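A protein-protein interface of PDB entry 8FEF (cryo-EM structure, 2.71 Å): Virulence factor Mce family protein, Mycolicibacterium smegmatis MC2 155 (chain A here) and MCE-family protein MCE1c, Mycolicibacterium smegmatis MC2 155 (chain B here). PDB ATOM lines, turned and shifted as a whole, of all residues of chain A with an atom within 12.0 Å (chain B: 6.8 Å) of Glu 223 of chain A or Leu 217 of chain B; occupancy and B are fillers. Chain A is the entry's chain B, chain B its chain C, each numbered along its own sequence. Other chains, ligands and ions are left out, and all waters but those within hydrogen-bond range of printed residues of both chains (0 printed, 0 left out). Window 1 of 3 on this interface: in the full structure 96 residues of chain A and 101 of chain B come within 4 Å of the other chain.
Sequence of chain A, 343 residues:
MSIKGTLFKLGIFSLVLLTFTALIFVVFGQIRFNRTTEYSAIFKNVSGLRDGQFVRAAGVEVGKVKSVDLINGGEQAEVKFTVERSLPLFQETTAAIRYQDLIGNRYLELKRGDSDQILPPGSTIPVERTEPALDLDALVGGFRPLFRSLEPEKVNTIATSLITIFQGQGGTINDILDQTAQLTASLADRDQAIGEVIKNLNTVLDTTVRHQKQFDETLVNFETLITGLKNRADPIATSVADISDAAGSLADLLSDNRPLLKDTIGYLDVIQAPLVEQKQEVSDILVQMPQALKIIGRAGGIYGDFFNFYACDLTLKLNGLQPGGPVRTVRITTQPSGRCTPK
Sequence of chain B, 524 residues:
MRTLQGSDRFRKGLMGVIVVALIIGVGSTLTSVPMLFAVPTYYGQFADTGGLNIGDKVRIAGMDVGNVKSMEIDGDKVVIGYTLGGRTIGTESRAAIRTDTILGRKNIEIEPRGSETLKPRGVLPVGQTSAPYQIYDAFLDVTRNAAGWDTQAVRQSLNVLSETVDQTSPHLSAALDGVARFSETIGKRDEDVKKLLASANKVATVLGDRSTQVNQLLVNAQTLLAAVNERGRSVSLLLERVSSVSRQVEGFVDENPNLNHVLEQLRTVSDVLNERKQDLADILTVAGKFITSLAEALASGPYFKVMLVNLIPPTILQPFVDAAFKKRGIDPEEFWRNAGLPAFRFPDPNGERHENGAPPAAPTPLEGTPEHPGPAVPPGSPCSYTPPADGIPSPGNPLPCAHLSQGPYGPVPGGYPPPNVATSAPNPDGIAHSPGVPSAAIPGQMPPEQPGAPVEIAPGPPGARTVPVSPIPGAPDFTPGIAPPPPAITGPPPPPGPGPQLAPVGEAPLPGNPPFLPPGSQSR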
ATOM      1  N   GLN A 214      16.416   6.334  -2.605  1.00  0.00           N
ATOM      2  CA  GLN A 214      15.707   5.606  -3.651  1.00  0.00           C
ATOM      3  C   GLN A 214      16.653   4.721  -4.453  1.00  0.00           C
ATOM      4  O   GLN A 214      16.293   3.597  -4.822  1.00  0.00           O
ATOM      5  CB  GLN A 214      14.983   6.589  -4.570  1.00  0.00           C
ATOM      6  CG  GLN A 214      14.349   7.766  -3.845  1.00  0.00           C
ATOM      7  CD  GLN A 214      13.410   7.336  -2.734  1.00  0.00           C
ATOM      8  OE1 GLN A 214      12.625   6.402  -2.893  1.00  0.00           O
ATOM      9  NE2 GLN A 214      13.491   8.017  -1.597  1.00  0.00           N
ATOM     10  N   PHE A 215      17.861   5.213  -4.737  1.00  0.00           N
ATOM     11  CA  PHE A 215      18.849   4.408  -5.449  1.00  0.00           C
ATOM     12  C   PHE A 215      19.252   3.176  -4.648  1.00  0.00           C
ATOM     13  O   PHE A 215      19.557   2.130  -5.229  1.00  0.00           O
ATOM     14  CB  PHE A 215      20.071   5.266  -5.777  1.00  0.00           C
ATOM     15  CG  PHE A 215      21.204   4.506  -6.400  1.00  0.00           C
ATOM     16  CD1 PHE A 215      21.092   3.993  -7.680  1.00  0.00           C
ATOM     17  CD2 PHE A 215      22.391   4.320  -5.712  1.00  0.00           C
ATOM     18  CE1 PHE A 215      22.136   3.298  -8.257  1.00  0.00           C
ATOM     19  CE2 PHE A 215      23.439   3.627  -6.285  1.00  0.00           C
ATOM     20  CZ  PHE A 215      23.311   3.117  -7.558  1.00  0.00           C
ATOM     21  N   ASP A 216      19.270   3.282  -3.319  1.00  0.00           N
ATOM     22  CA  ASP A 216      19.578   2.127  -2.484  1.00  0.00           C
ATOM     23  C   ASP A 216      18.409   1.153  -2.435  1.00  0.00           C
ATOM     24  O   ASP A 216      18.607  -0.064  -2.513  1.00  0.00           O
ATOM     25  CB  ASP A 216      19.952   2.591  -1.076  1.00  0.00           C
ATOM     26  CG  ASP A 216      20.234   1.437  -0.137  1.00  0.00           C
ATOM     27  OD1 ASP A 216      21.350   0.881  -0.195  1.00  0.00           O
ATOM     28  OD2 ASP A 216      19.341   1.086   0.663  1.00  0.00           O
ATOM     29  N   GLU A 217      17.184   1.669  -2.299  1.00  0.00           N
ATOM     30  CA  GLU A 217      16.020   0.790  -2.200  1.00  0.00           C
ATOM     31  C   GLU A 217      15.719   0.072  -3.511  1.00  0.00           C
ATOM     32  O   GLU A 217      15.236  -1.071  -3.489  1.00  0.00           O
ATOM     33  CB  GLU A 217      14.793   1.583  -1.751  1.00  0.00           C
ATOM     34  CG  GLU A 217      14.874   2.119  -0.334  1.00  0.00           C
ATOM     35  CD  GLU A 217      13.599   2.821   0.091  1.00  0.00           C
ATOM     36  OE1 GLU A 217      12.595   2.731  -0.646  1.00  0.00           O
ATOM     37  OE2 GLU A 217      13.599   3.461   1.162  1.00  0.00           O
ATOM     38  N   THR A 218      15.977   0.717  -4.653  1.00  0.00           N
ATOM     39  CA  THR A 218      15.593   0.120  -5.926  1.00  0.00           C
ATOM     40  C   THR A 218      16.419  -1.118  -6.248  1.00  0.00           C
ATOM     41  O   THR A 218      15.914  -2.028  -6.905  1.00  0.00           O
ATOM     42  CB  THR A 218      15.691   1.144  -7.062  1.00  0.00           C
ATOM     43  OG1 THR A 218      15.228   0.548  -8.279  1.00  0.00           O
ATOM     44  CG2 THR A 218      17.118   1.619  -7.263  1.00  0.00           C
ATOM     45  N   LEU A 219      17.671  -1.187  -5.786  1.00  0.00           N
ATOM     46  CA  LEU A 219      18.471  -2.390  -6.008  1.00  0.00           C
ATOM     47  C   LEU A 219      17.846  -3.595  -5.314  1.00  0.00           C
ATOM     48  O   LEU A 219      17.680  -4.660  -5.920  1.00  0.00           O
ATOM     49  CB  LEU A 219      19.902  -2.171  -5.519  1.00  0.00           C
ATOM     50  CG  LEU A 219      20.696  -1.055  -6.195  1.00  0.00           C
ATOM     51  CD1 LEU A 219      22.104  -0.989  -5.629  1.00  0.00           C
ATOM     52  CD2 LEU A 219      20.727  -1.261  -7.698  1.00  0.00           C
ATOM     53  N   VAL A 220      17.480  -3.435  -4.041  1.00  0.00           N
ATOM     54  CA  VAL A 220      16.869  -4.528  -3.292  1.00  0.00           C
ATOM     55  C   VAL A 220      15.512  -4.892  -3.881  1.00  0.00           C
ATOM     56  O   VAL A 220      15.172  -6.076  -4.003  1.00  0.00           O
ATOM     57  CB  VAL A 220      16.756  -4.155  -1.803  1.00  0.00           C
ATOM     58  CG1 VAL A 220      16.299  -5.354  -0.988  1.00  0.00           C
ATOM     59  CG2 VAL A 220      18.082  -3.624  -1.291  1.00  0.00           C
ATOM     60  N   ASN A 221      14.709  -3.886  -4.245  1.00  0.00           N
ATOM     61  CA  ASN A 221      13.394  -4.170  -4.812  1.00  0.00           C
ATOM     62  C   ASN A 221      13.509  -4.891  -6.150  1.00  0.00           C
ATOM     63  O   ASN A 221      12.757  -5.837  -6.422  1.00  0.00           O
ATOM     64  CB  ASN A 221      12.593  -2.878  -4.962  1.00  0.00           C
ATOM     65  CG  ASN A 221      12.216  -2.269  -3.628  1.00  0.00           C
ATOM     66  OD1 ASN A 221      12.386  -1.071  -3.409  1.00  0.00           O
ATOM     67  ND2 ASN A 221      11.702  -3.095  -2.725  1.00  0.00           N
ATOM     68  N   PHE A 222      14.446  -4.461  -6.998  1.00  0.00           N
ATOM     69  CA  PHE A 222      14.657  -5.117  -8.280  1.00  0.00           C
ATOM     70  C   PHE A 222      15.148  -6.544  -8.090  1.00  0.00           C
ATOM     71  O   PHE A 222      14.719  -7.454  -8.807  1.00  0.00           O
ATOM     72  CB  PHE A 222      15.652  -4.314  -9.114  1.00  0.00           C
ATOM     73  CG  PHE A 222      15.376  -4.344 -10.586  1.00  0.00           C
ATOM     74  CD1 PHE A 222      14.412  -5.188 -11.109  1.00  0.00           C
ATOM     75  CD2 PHE A 222      16.085  -3.528 -11.451  1.00  0.00           C
ATOM     76  CE1 PHE A 222      14.157  -5.215 -12.461  1.00  0.00           C
ATOM     77  CE2 PHE A 222      15.834  -3.553 -12.804  1.00  0.00           C
ATOM     78  CZ  PHE A 222      14.871  -4.399 -13.311  1.00  0.00           C
ATOM     79  N   GLU A 223      16.053  -6.757  -7.131  1.00  0.00           N
ATOM     80  CA  GLU A 223      16.526  -8.106  -6.847  1.00  0.00           C
ATOM     81  C   GLU A 223      15.383  -9.003  -6.395  1.00  0.00           C
ATOM     82  O   GLU A 223      15.266 -10.145  -6.854  1.00  0.00           O
ATOM     83  CB  GLU A 223      17.635  -8.064  -5.795  1.00  0.00           C
ATOM     84  CG  GLU A 223      18.237  -9.420  -5.440  1.00  0.00           C
ATOM     85  CD  GLU A 223      17.526 -10.108  -4.289  1.00  0.00           C
ATOM     86  OE1 GLU A 223      16.879  -9.407  -3.483  1.00  0.00           O
ATOM     87  OE2 GLU A 223      17.611 -11.350  -4.191  1.00  0.00           O
ATOM     88  N   THR A 224      14.525  -8.501  -5.504  1.00  0.00           N
ATOM     89  CA  THR A 224      13.393  -9.295  -5.034  1.00  0.00           C
ATOM     90  C   THR A 224      12.444  -9.632  -6.177  1.00  0.00           C
ATOM     91  O   THR A 224      12.010 -10.782  -6.321  1.00  0.00           O
ATOM     92  CB  THR A 224      12.651  -8.545  -3.928  1.00  0.00           C
ATOM     93  OG1 THR A 224      13.574  -8.173  -2.897  1.00  0.00           O
ATOM     94  CG2 THR A 224      11.561  -9.419  -3.332  1.00  0.00           C
ATOM     95  N   LEU A 225      12.123  -8.639  -7.012  1.00  0.00           N
ATOM     96  CA  LEU A 225      11.209  -8.864  -8.129  1.00  0.00           C
ATOM     97  C   LEU A 225      11.780  -9.876  -9.116  1.00  0.00           C
ATOM     98  O   LEU A 225      11.081 -10.797  -9.557  1.00  0.00           O
ATOM     99  CB  LEU A 225      10.917  -7.537  -8.829  1.00  0.00           C
ATOM    100  CG  LEU A 225      10.242  -7.603 -10.199  1.00  0.00           C
ATOM    101  CD1 LEU A 225       8.840  -8.171 -10.085  1.00  0.00           C
ATOM    102  CD2 LEU A 225      10.218  -6.231 -10.842  1.00  0.00           C
ATOM    103  N   ILE A 226      13.060  -9.725  -9.462  1.00  0.00           N
ATOM    104  CA  ILE A 226      13.672 -10.599 -10.455  1.00  0.00           C
ATOM    105  C   ILE A 226      13.828 -12.013  -9.910  1.00  0.00           C
ATOM    106  O   ILE A 226      13.631 -12.990 -10.638  1.00  0.00           O
ATOM    107  CB  ILE A 226      15.007 -10.000 -10.931  1.00  0.00           C
ATOM    108  CG1 ILE A 226      14.738  -8.779 -11.810  1.00  0.00           C
ATOM    109  CG2 ILE A 226      15.821 -11.022 -11.688  1.00  0.00           C
ATOM    110  CD1 ILE A 226      15.938  -8.303 -12.589  1.00  0.00           C
ATOM    111  N   THR A 227      14.170 -12.154  -8.626  1.00  0.00           N
ATOM    112  CA  THR A 227      14.244 -13.485  -8.030  1.00  0.00           C
ATOM    113  C   THR A 227      12.874 -14.153  -8.002  1.00  0.00           C
ATOM    114  O   THR A 227      12.749 -15.348  -8.304  1.00  0.00           O
ATOM    115  CB  THR A 227      14.832 -13.395  -6.621  1.00  0.00           C
ATOM    116  OG1 THR A 227      16.172 -12.893  -6.694  1.00  0.00           O
ATOM    117  CG2 THR A 227      14.849 -14.760  -5.955  1.00  0.00           C
ATOM    118  N   GLY A 228      11.832 -13.397  -7.642  1.00  0.00           N
ATOM    119  CA  GLY A 228      10.491 -13.956  -7.640  1.00  0.00           C
ATOM    120  C   GLY A 228      10.035 -14.386  -9.021  1.00  0.00           C
ATOM    121  O   GLY A 228       9.349 -15.400  -9.171  1.00  0.00           O
ATOM    122  N   LEU A 229      10.402 -13.616 -10.047  1.00  0.00           N
ATOM    123  CA  LEU A 229      10.080 -14.015 -11.414  1.00  0.00           C
ATOM    124  C   LEU A 229      10.906 -15.217 -11.863  1.00  0.00           C
ATOM    125  O   LEU A 229      10.397 -16.093 -12.569  1.00  0.00           O
ATOM    126  CB  LEU A 229      10.284 -12.840 -12.368  1.00  0.00           C
ATOM    127  CG  LEU A 229       9.340 -11.648 -12.212  1.00  0.00           C
ATOM    128  CD1 LEU A 229       9.624 -10.607 -13.279  1.00  0.00           C
ATOM    129  CD2 LEU A 229       7.893 -12.101 -12.275  1.00  0.00           C
ATOM    130  N   LYS A 230      12.182 -15.272 -11.478  1.00  0.00           N
ATOM    131  CA  LYS A 230      13.035 -16.390 -11.873  1.00  0.00           C
ATOM    132  C   LYS A 230      12.561 -17.696 -11.248  1.00  0.00           C
ATOM    133  O   LYS A 230      12.643 -18.756 -11.878  1.00  0.00           O
ATOM    134  CB  LYS A 230      14.488 -16.089 -11.494  1.00  0.00           C
ATOM    135  CG  LYS A 230      15.430 -17.286 -11.483  1.00  0.00           C
ATOM    136  CD  LYS A 230      15.738 -17.739 -10.062  1.00  0.00           C
ATOM    137  CE  LYS A 230      16.613 -18.978 -10.050  1.00  0.00           C
ATOM    138  NZ  LYS A 230      16.870 -19.459  -8.666  1.00  0.00           N
ATOM    139  N   ASN A 231      12.049 -17.638 -10.016  1.00  0.00           N
ATOM    140  CA  ASN A 231      11.554 -18.846  -9.363  1.00  0.00           C
ATOM    141  C   ASN A 231      10.333 -19.441 -10.056  1.00  0.00           C
ATOM    142  O   ASN A 231       9.979 -20.589  -9.767  1.00  0.00           O
ATOM    143  CB  ASN A 231      11.227 -18.555  -7.899  1.00  0.00           C
ATOM    144  CG  ASN A 231      12.466 -18.306  -7.065  1.00  0.00           C
ATOM    145  OD1 ASN A 231      13.551 -18.075  -7.599  1.00  0.00           O
ATOM    146  ND2 ASN A 231      12.313 -18.352  -5.748  1.00  0.00           N
ATOM    147  N   ARG A 232       9.681 -18.692 -10.952  1.00  0.00           N
ATOM    148  CA  ARG A 232       8.543 -19.180 -11.723  1.00  0.00           C
ATOM    149  C   ARG A 232       8.746 -18.954 -13.218  1.00  0.00           C
ATOM    150  O   ARG A 232       7.768 -18.929 -13.970  1.00  0.00           O
ATOM    151  CB  ARG A 232       7.244 -18.516 -11.260  1.00  0.00           C
ATOM    152  CG  ARG A 232       7.038 -18.537  -9.755  1.00  0.00           C
ATOM    153  CD  ARG A 232       5.748 -17.845  -9.354  1.00  0.00           C
ATOM    154  NE  ARG A 232       4.577 -18.534  -9.881  1.00  0.00           N
ATOM    155  CZ  ARG A 232       3.327 -18.251  -9.542  1.00  0.00           C
ATOM    156  NH1 ARG A 232       3.045 -17.300  -8.667  1.00  0.00           N
ATOM    157  NH2 ARG A 232       2.333 -18.944 -10.093  1.00  0.00           N
ATOM    158  N   ALA A 233       9.995 -18.731 -13.637  1.00  0.00           N
ATOM    159  CA  ALA A 233      10.317 -18.443 -15.034  1.00  0.00           C
ATOM    160  C   ALA A 233       9.717 -19.457 -16.001  1.00  0.00           C
ATOM    161  O   ALA A 233       9.117 -19.076 -17.013  1.00  0.00           O
ATOM    162  CB  ALA A 233      11.836 -18.386 -15.206  1.00  0.00           C
ATOM    163  N   ARG B 210      25.008  -3.449  -1.180  1.00  0.00           N
ATOM    164  CA  ARG B 210      24.015  -4.209  -1.927  1.00  0.00           C
ATOM    165  C   ARG B 210      24.633  -5.012  -3.067  1.00  0.00           C
ATOM    166  O   ARG B 210      23.933  -5.366  -4.019  1.00  0.00           O
ATOM    167  CB  ARG B 210      22.938  -3.270  -2.471  1.00  0.00           C
ATOM    168  CG  ARG B 210      22.290  -2.394  -1.417  1.00  0.00           C
ATOM    169  CD  ARG B 210      21.607  -3.229  -0.352  1.00  0.00           C
ATOM    170  NE  ARG B 210      20.945  -2.399   0.646  1.00  0.00           N
ATOM    171  CZ  ARG B 210      20.243  -2.873   1.665  1.00  0.00           C
ATOM    172  NH1 ARG B 210      20.093  -4.173   1.856  1.00  0.00           N
ATOM    173  NH2 ARG B 210      19.676  -2.020   2.515  1.00  0.00           N
ATOM    174  N   SER B 211      25.933  -5.307  -2.988  1.00  0.00           N
ATOM    175  CA  SER B 211      26.615  -5.986  -4.087  1.00  0.00           C
ATOM    176  C   SER B 211      26.107  -7.410  -4.283  1.00  0.00           C
ATOM    177  O   SER B 211      25.960  -7.870  -5.425  1.00  0.00           O
ATOM    178  CB  SER B 211      28.119  -5.990  -3.842  1.00  0.00           C
ATOM    179  OG  SER B 211      28.779  -6.646  -4.903  1.00  0.00           O
ATOM    180  N   THR B 212      25.857  -8.130  -3.188  1.00  0.00           N
ATOM    181  CA  THR B 212      25.305  -9.477  -3.298  1.00  0.00           C
ATOM    182  C   THR B 212      23.946  -9.448  -3.982  1.00  0.00           C
ATOM    183  O   THR B 212      23.653 -10.288  -4.844  1.00  0.00           O
ATOM    184  CB  THR B 212      25.202 -10.117  -1.913  1.00  0.00           C
ATOM    185  OG1 THR B 212      26.498 -10.159  -1.306  1.00  0.00           O
ATOM    186  CG2 THR B 212      24.656 -11.531  -2.014  1.00  0.00           C
ATOM    187  N   GLN B 213      23.107  -8.474  -3.617  1.00  0.00           N
ATOM    188  CA  GLN B 213      21.822  -8.304  -4.281  1.00  0.00           C
ATOM    189  C   GLN B 213      22.005  -8.001  -5.761  1.00  0.00           C
ATOM    190  O   GLN B 213      21.246  -8.499  -6.598  1.00  0.00           O
ATOM    191  CB  GLN B 213      21.018  -7.195  -3.603  1.00  0.00           C
ATOM    192  CG  GLN B 213      20.304  -7.619  -2.327  1.00  0.00           C
ATOM    193  CD  GLN B 213      21.245  -7.809  -1.155  1.00  0.00           C
ATOM    194  OE1 GLN B 213      22.405  -7.401  -1.199  1.00  0.00           O
ATOM    195  NE2 GLN B 213      20.746  -8.433  -0.093  1.00  0.00           N
ATOM    196  N   VAL B 214      23.007  -7.186  -6.104  1.00  0.00           N
ATOM    197  CA  VAL B 214      23.256  -6.851  -7.505  1.00  0.00           C
ATOM    198  C   VAL B 214      23.599  -8.105  -8.300  1.00  0.00           C
ATOM    199  O   VAL B 214      23.027  -8.363  -9.366  1.00  0.00           O
ATOM    200  CB  VAL B 214      24.365  -5.791  -7.619  1.00  0.00           C
ATOM    201  CG1 VAL B 214      24.829  -5.664  -9.056  1.00  0.00           C
ATOM    202  CG2 VAL B 214      23.868  -4.451  -7.117  1.00  0.00           C
ATOM    203  N   ASN B 215      24.536  -8.907  -7.787  1.00  0.00           N
ATOM    204  CA  ASN B 215      24.951 -10.108  -8.508  1.00  0.00           C
ATOM    205  C   ASN B 215      23.806 -11.106  -8.621  1.00  0.00           C
ATOM    206  O   ASN B 215      23.607 -11.722  -9.679  1.00  0.00           O
ATOM    207  CB  ASN B 215      26.154 -10.748  -7.817  1.00  0.00           C
ATOM    208  CG  ASN B 215      26.839 -11.785  -8.682  1.00  0.00           C
ATOM    209  OD1 ASN B 215      26.582 -11.879  -9.883  1.00  0.00           O
ATOM    210  ND2 ASN B 215      27.721 -12.571  -8.077  1.00  0.00           N
ATOM    211  N   GLN B 216      23.043 -11.280  -7.539  1.00  0.00           N
ATOM    212  CA  GLN B 216      21.923 -12.211  -7.564  1.00  0.00           C
ATOM    213  C   GLN B 216      20.852 -11.759  -8.549  1.00  0.00           C
ATOM    214  O   GLN B 216      20.294 -12.578  -9.290  1.00  0.00           O
ATOM    215  CB  GLN B 216      21.343 -12.362  -6.158  1.00  0.00           C
ATOM    216  CG  GLN B 216      20.412 -13.542  -5.988  1.00  0.00           C
ATOM    217  CD  GLN B 216      20.127 -13.843  -4.532  1.00  0.00           C
ATOM    218  OE1 GLN B 216      20.857 -13.407  -3.643  1.00  0.00           O
ATOM    219  NE2 GLN B 216      19.059 -14.590  -4.280  1.00  0.00           N
ATOM    220  N   LEU B 217      20.556 -10.455  -8.580  1.00  0.00           N
ATOM    221  CA  LEU B 217      19.585  -9.938  -9.535  1.00  0.00           C
ATOM    222  C   LEU B 217      20.066 -10.133 -10.966  1.00  0.00           C
ATOM    223  O   LEU B 217      19.276 -10.490 -11.844  1.00  0.00           O
ATOM    224  CB  LEU B 217      19.285  -8.462  -9.238  1.00  0.00           C
ATOM    225  CG  LEU B 217      19.865  -7.291 -10.045  1.00  0.00           C
ATOM    226  CD1 LEU B 217      18.989  -6.925 -11.230  1.00  0.00           C
ATOM    227  CD2 LEU B 217      20.062  -6.080  -9.154  1.00  0.00           C
ATOM    228  N   LEU B 218      21.360  -9.919 -11.220  1.00  0.00           N
ATOM    229  CA  LEU B 218      21.881 -10.095 -12.574  1.00  0.00           C
ATOM    230  C   LEU B 218      21.770 -11.548 -13.027  1.00  0.00           C
ATOM    231  O   LEU B 218      21.304 -11.829 -14.141  1.00  0.00           O
ATOM    232  CB  LEU B 218      23.328  -9.608 -12.651  1.00  0.00           C
ATOM    233  CG  LEU B 218      23.528  -8.095 -12.545  1.00  0.00           C
ATOM    234  CD1 LEU B 218      24.990  -7.722 -12.709  1.00  0.00           C
ATOM    235  CD2 LEU B 218      22.673  -7.368 -13.565  1.00  0.00           C
ATOM    236  N   VAL B 219      22.181 -12.492 -12.174  1.00  0.00           N
ATOM    237  CA  VAL B 219      22.151 -13.893 -12.589  1.00  0.00           C
ATOM    238  C   VAL B 219      20.712 -14.390 -12.723  1.00  0.00           C
ATOM    239  O   VAL B 219      20.393 -15.161 -13.640  1.00  0.00           O
ATOM    240  CB  VAL B 219      22.992 -14.771 -11.640  1.00  0.00           C
ATOM    241  CG1 VAL B 219      24.443 -14.316 -11.652  1.00  0.00           C
ATOM    242  CG2 VAL B 219      22.447 -14.760 -10.226  1.00  0.00           C
ATOM    243  N   ASN B 220      19.815 -13.946 -11.836  1.00  0.00           N
ATOM    244  CA  ASN B 220      18.420 -14.359 -11.945  1.00  0.00           C
ATOM    245  C   ASN B 220      17.758 -13.745 -13.172  1.00  0.00           C
ATOM    246  O   ASN B 220      16.904 -14.378 -13.801  1.00  0.00           O
ATOM    247  CB  ASN B 220      17.661 -13.990 -10.674  1.00  0.00           C
ATOM    248  CG  ASN B 220      18.142 -14.765  -9.469  1.00  0.00           C
ATOM    249  OD1 ASN B 220      18.522 -15.929  -9.578  1.00  0.00           O
ATOM    250  ND2 ASN B 220      18.127 -14.123  -8.310  1.00  0.00           N
ATOM    251  N   ALA B 221      18.136 -12.514 -13.526  1.00  0.00           N
ATOM    252  CA  ALA B 221      17.641 -11.914 -14.758  1.00  0.00           C
ATOM    253  C   ALA B 221      18.114 -12.696 -15.971  1.00  0.00           C
ATOM    254  O   ALA B 221      17.350 -12.901 -16.920  1.00  0.00           O
ATOM    255  CB  ALA B 221      18.086 -10.455 -14.847  1.00  0.00           C
ATOM    256  N   GLN B 222      19.375 -13.140 -15.960  1.00  0.00           N
ATOM    257  CA  GLN B 222      19.874 -13.973 -17.051  1.00  0.00           C
ATOM    258  C   GLN B 222      19.074 -15.266 -17.160  1.00  0.00           C
ATOM    259  O   GLN B 222      18.680 -15.676 -18.260  1.00  0.00           O
ATOM    260  CB  GLN B 222      21.361 -14.271 -16.843  1.00  0.00           C
ATOM    261  CG  GLN B 222      22.058 -14.969 -18.011  1.00  0.00           C
ATOM    262  CD  GLN B 222      21.863 -16.475 -18.018  1.00  0.00           C
ATOM    263  OE1 GLN B 222      21.688 -17.095 -16.969  1.00  0.00           O
ATOM    264  NE2 GLN B 222      21.887 -17.068 -19.204  1.00  0.00           N
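Of the 20 printed residues of chain A, 7 touch a printed residue of chain B.
Printed residues of chain A that touch a printed residue of chain B: Asp 216, Leu 219, Val 220, Glu 223, Ile 226, Thr 227 and Lys 230.
Hydrophobic or aromatic side chains of chain A within 4 Å of the printed part of chain B: Leu 219, Val 220 and Ile 226.
Printed residues of chain B that touch a printed residue of chain A: Arg 210, Gln 213, Gln 216, Leu 217, Asn 220 and Ala 221.
Among the printed residues, 11 pairs touch across the chains.
Among the printed residues, Asp or Glu carboxylates within 4 Å of a Lys or Arg side-chain nitrogen of the other chain: Asp 216 of chain A with Arg 210 of chain B (3.4 Å).
The side-chain hydroxyl (OG1) of Thr 224 of chain A lies within hydrogen-bond range of the backbone carbonyl oxygen (O) of Val 220 of chain A.
O of Glu 223 of chain A sits at hydrogen-bond distance from OG1 of Thr 227 of chain A (2.9 Å).
O of Thr 227 of chain A lies close to OD1 of Asn 231 of chain A (2.9 Å).
The backbone carbonyl oxygen (O) of Gln 216 of chain B is in hydrogen-bond range of the side-chain amide nitrogen (ND2) of Asn 220 of chain B (2.8 Å).
Arg 210 of chain B touches Leu 219 of chain A (CB to CD1, 3.98 Å).
NE of Arg 210 of chain B touches CG2 of Val 220 of chain A, 3.7 Å away.
Glu 223 of chain A touches Gln 213 of chain B (CG to O, 3.4 Å).
OE2 of Glu 223 of chain A touches NE2 of Gln 216 of chain B, 3.5 Å away.
Glu 223 of chain A touches Leu 217 of chain B (CA to CB, 3.7 Å).
Ile 226 of chain A touches Leu 217 of chain B.
CG2 of Ile 226 of chain A touches CB of Asn 220 of chain B (3.6 Å).
Ile 226 of chain A touches Ala 221 of chain B.
Lys 230 of chain A touches Asn 220 of chain B (CD to OD1, 3.4 Å).
The side-chain carboxylate (OD1) of Asp 216 of chain A is in salt-bridge range of the guanidinium group (NE) of Arg 210 of chain B, 3.4 Å away.
The side-chain hydroxyl (OG1) of Thr 227 of chain A is in hydrogen-bond range of the side-chain amide nitrogen (ND2) of Asn 220 of chain B (2.8 Å).
Printed residues of chain B within 4 Å of Asp 216 of chain A: Arg 210 (3.4 Å).
Printed residues of chain B within 4 Å of Leu 219 of chain A: Arg 210.
Phe 222 of chain A touches none of the printed residues of chain B.
Printed residues of chain B within 4 Å of Glu 223 of chain A: Gln 213, Gln 216 and Leu 217.
Printed residues of chain B within 4 Å of Ile 226 of chain A: Leu 217, Asn 220 and Ala 221.
Of the printed residues of chain B, Thr 227 of chain A touches Asn 220.
Of the printed residues of chain B, Lys 230 of chain A touches Asn 220.
Of the printed residues of chain A, Gln 213 of chain B touches Glu 223.
Val 214 of chain B touches none of the printed residues of chain A.
No residue of chain A comes within 4 Å of Asn 215 of chain B.
Gln 216 of chain B touches just one residue of chain A: Glu 223 (3.5 Å).
Of chain A, only Glu 223 and Ile 226 come within 4 Å of Leu 217 of chain B.
No residue of chain A comes within 4 Å of Leu 218 of chain B.
No residue of chain A comes within 4 Å of Val 219 of chain B.
The nearest residue of chain B that does not touch Glu 223 of chain A is Asn 220 of chain B (5.0 Å).
The nearest residue of chain A that does not touch Leu 217 of chain B is Leu 219 of chain A (4.3 Å).
The nearest printed residue of chain B that does not touch Ile 226 of chain A is Gln 216 of chain B (5.3 Å).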
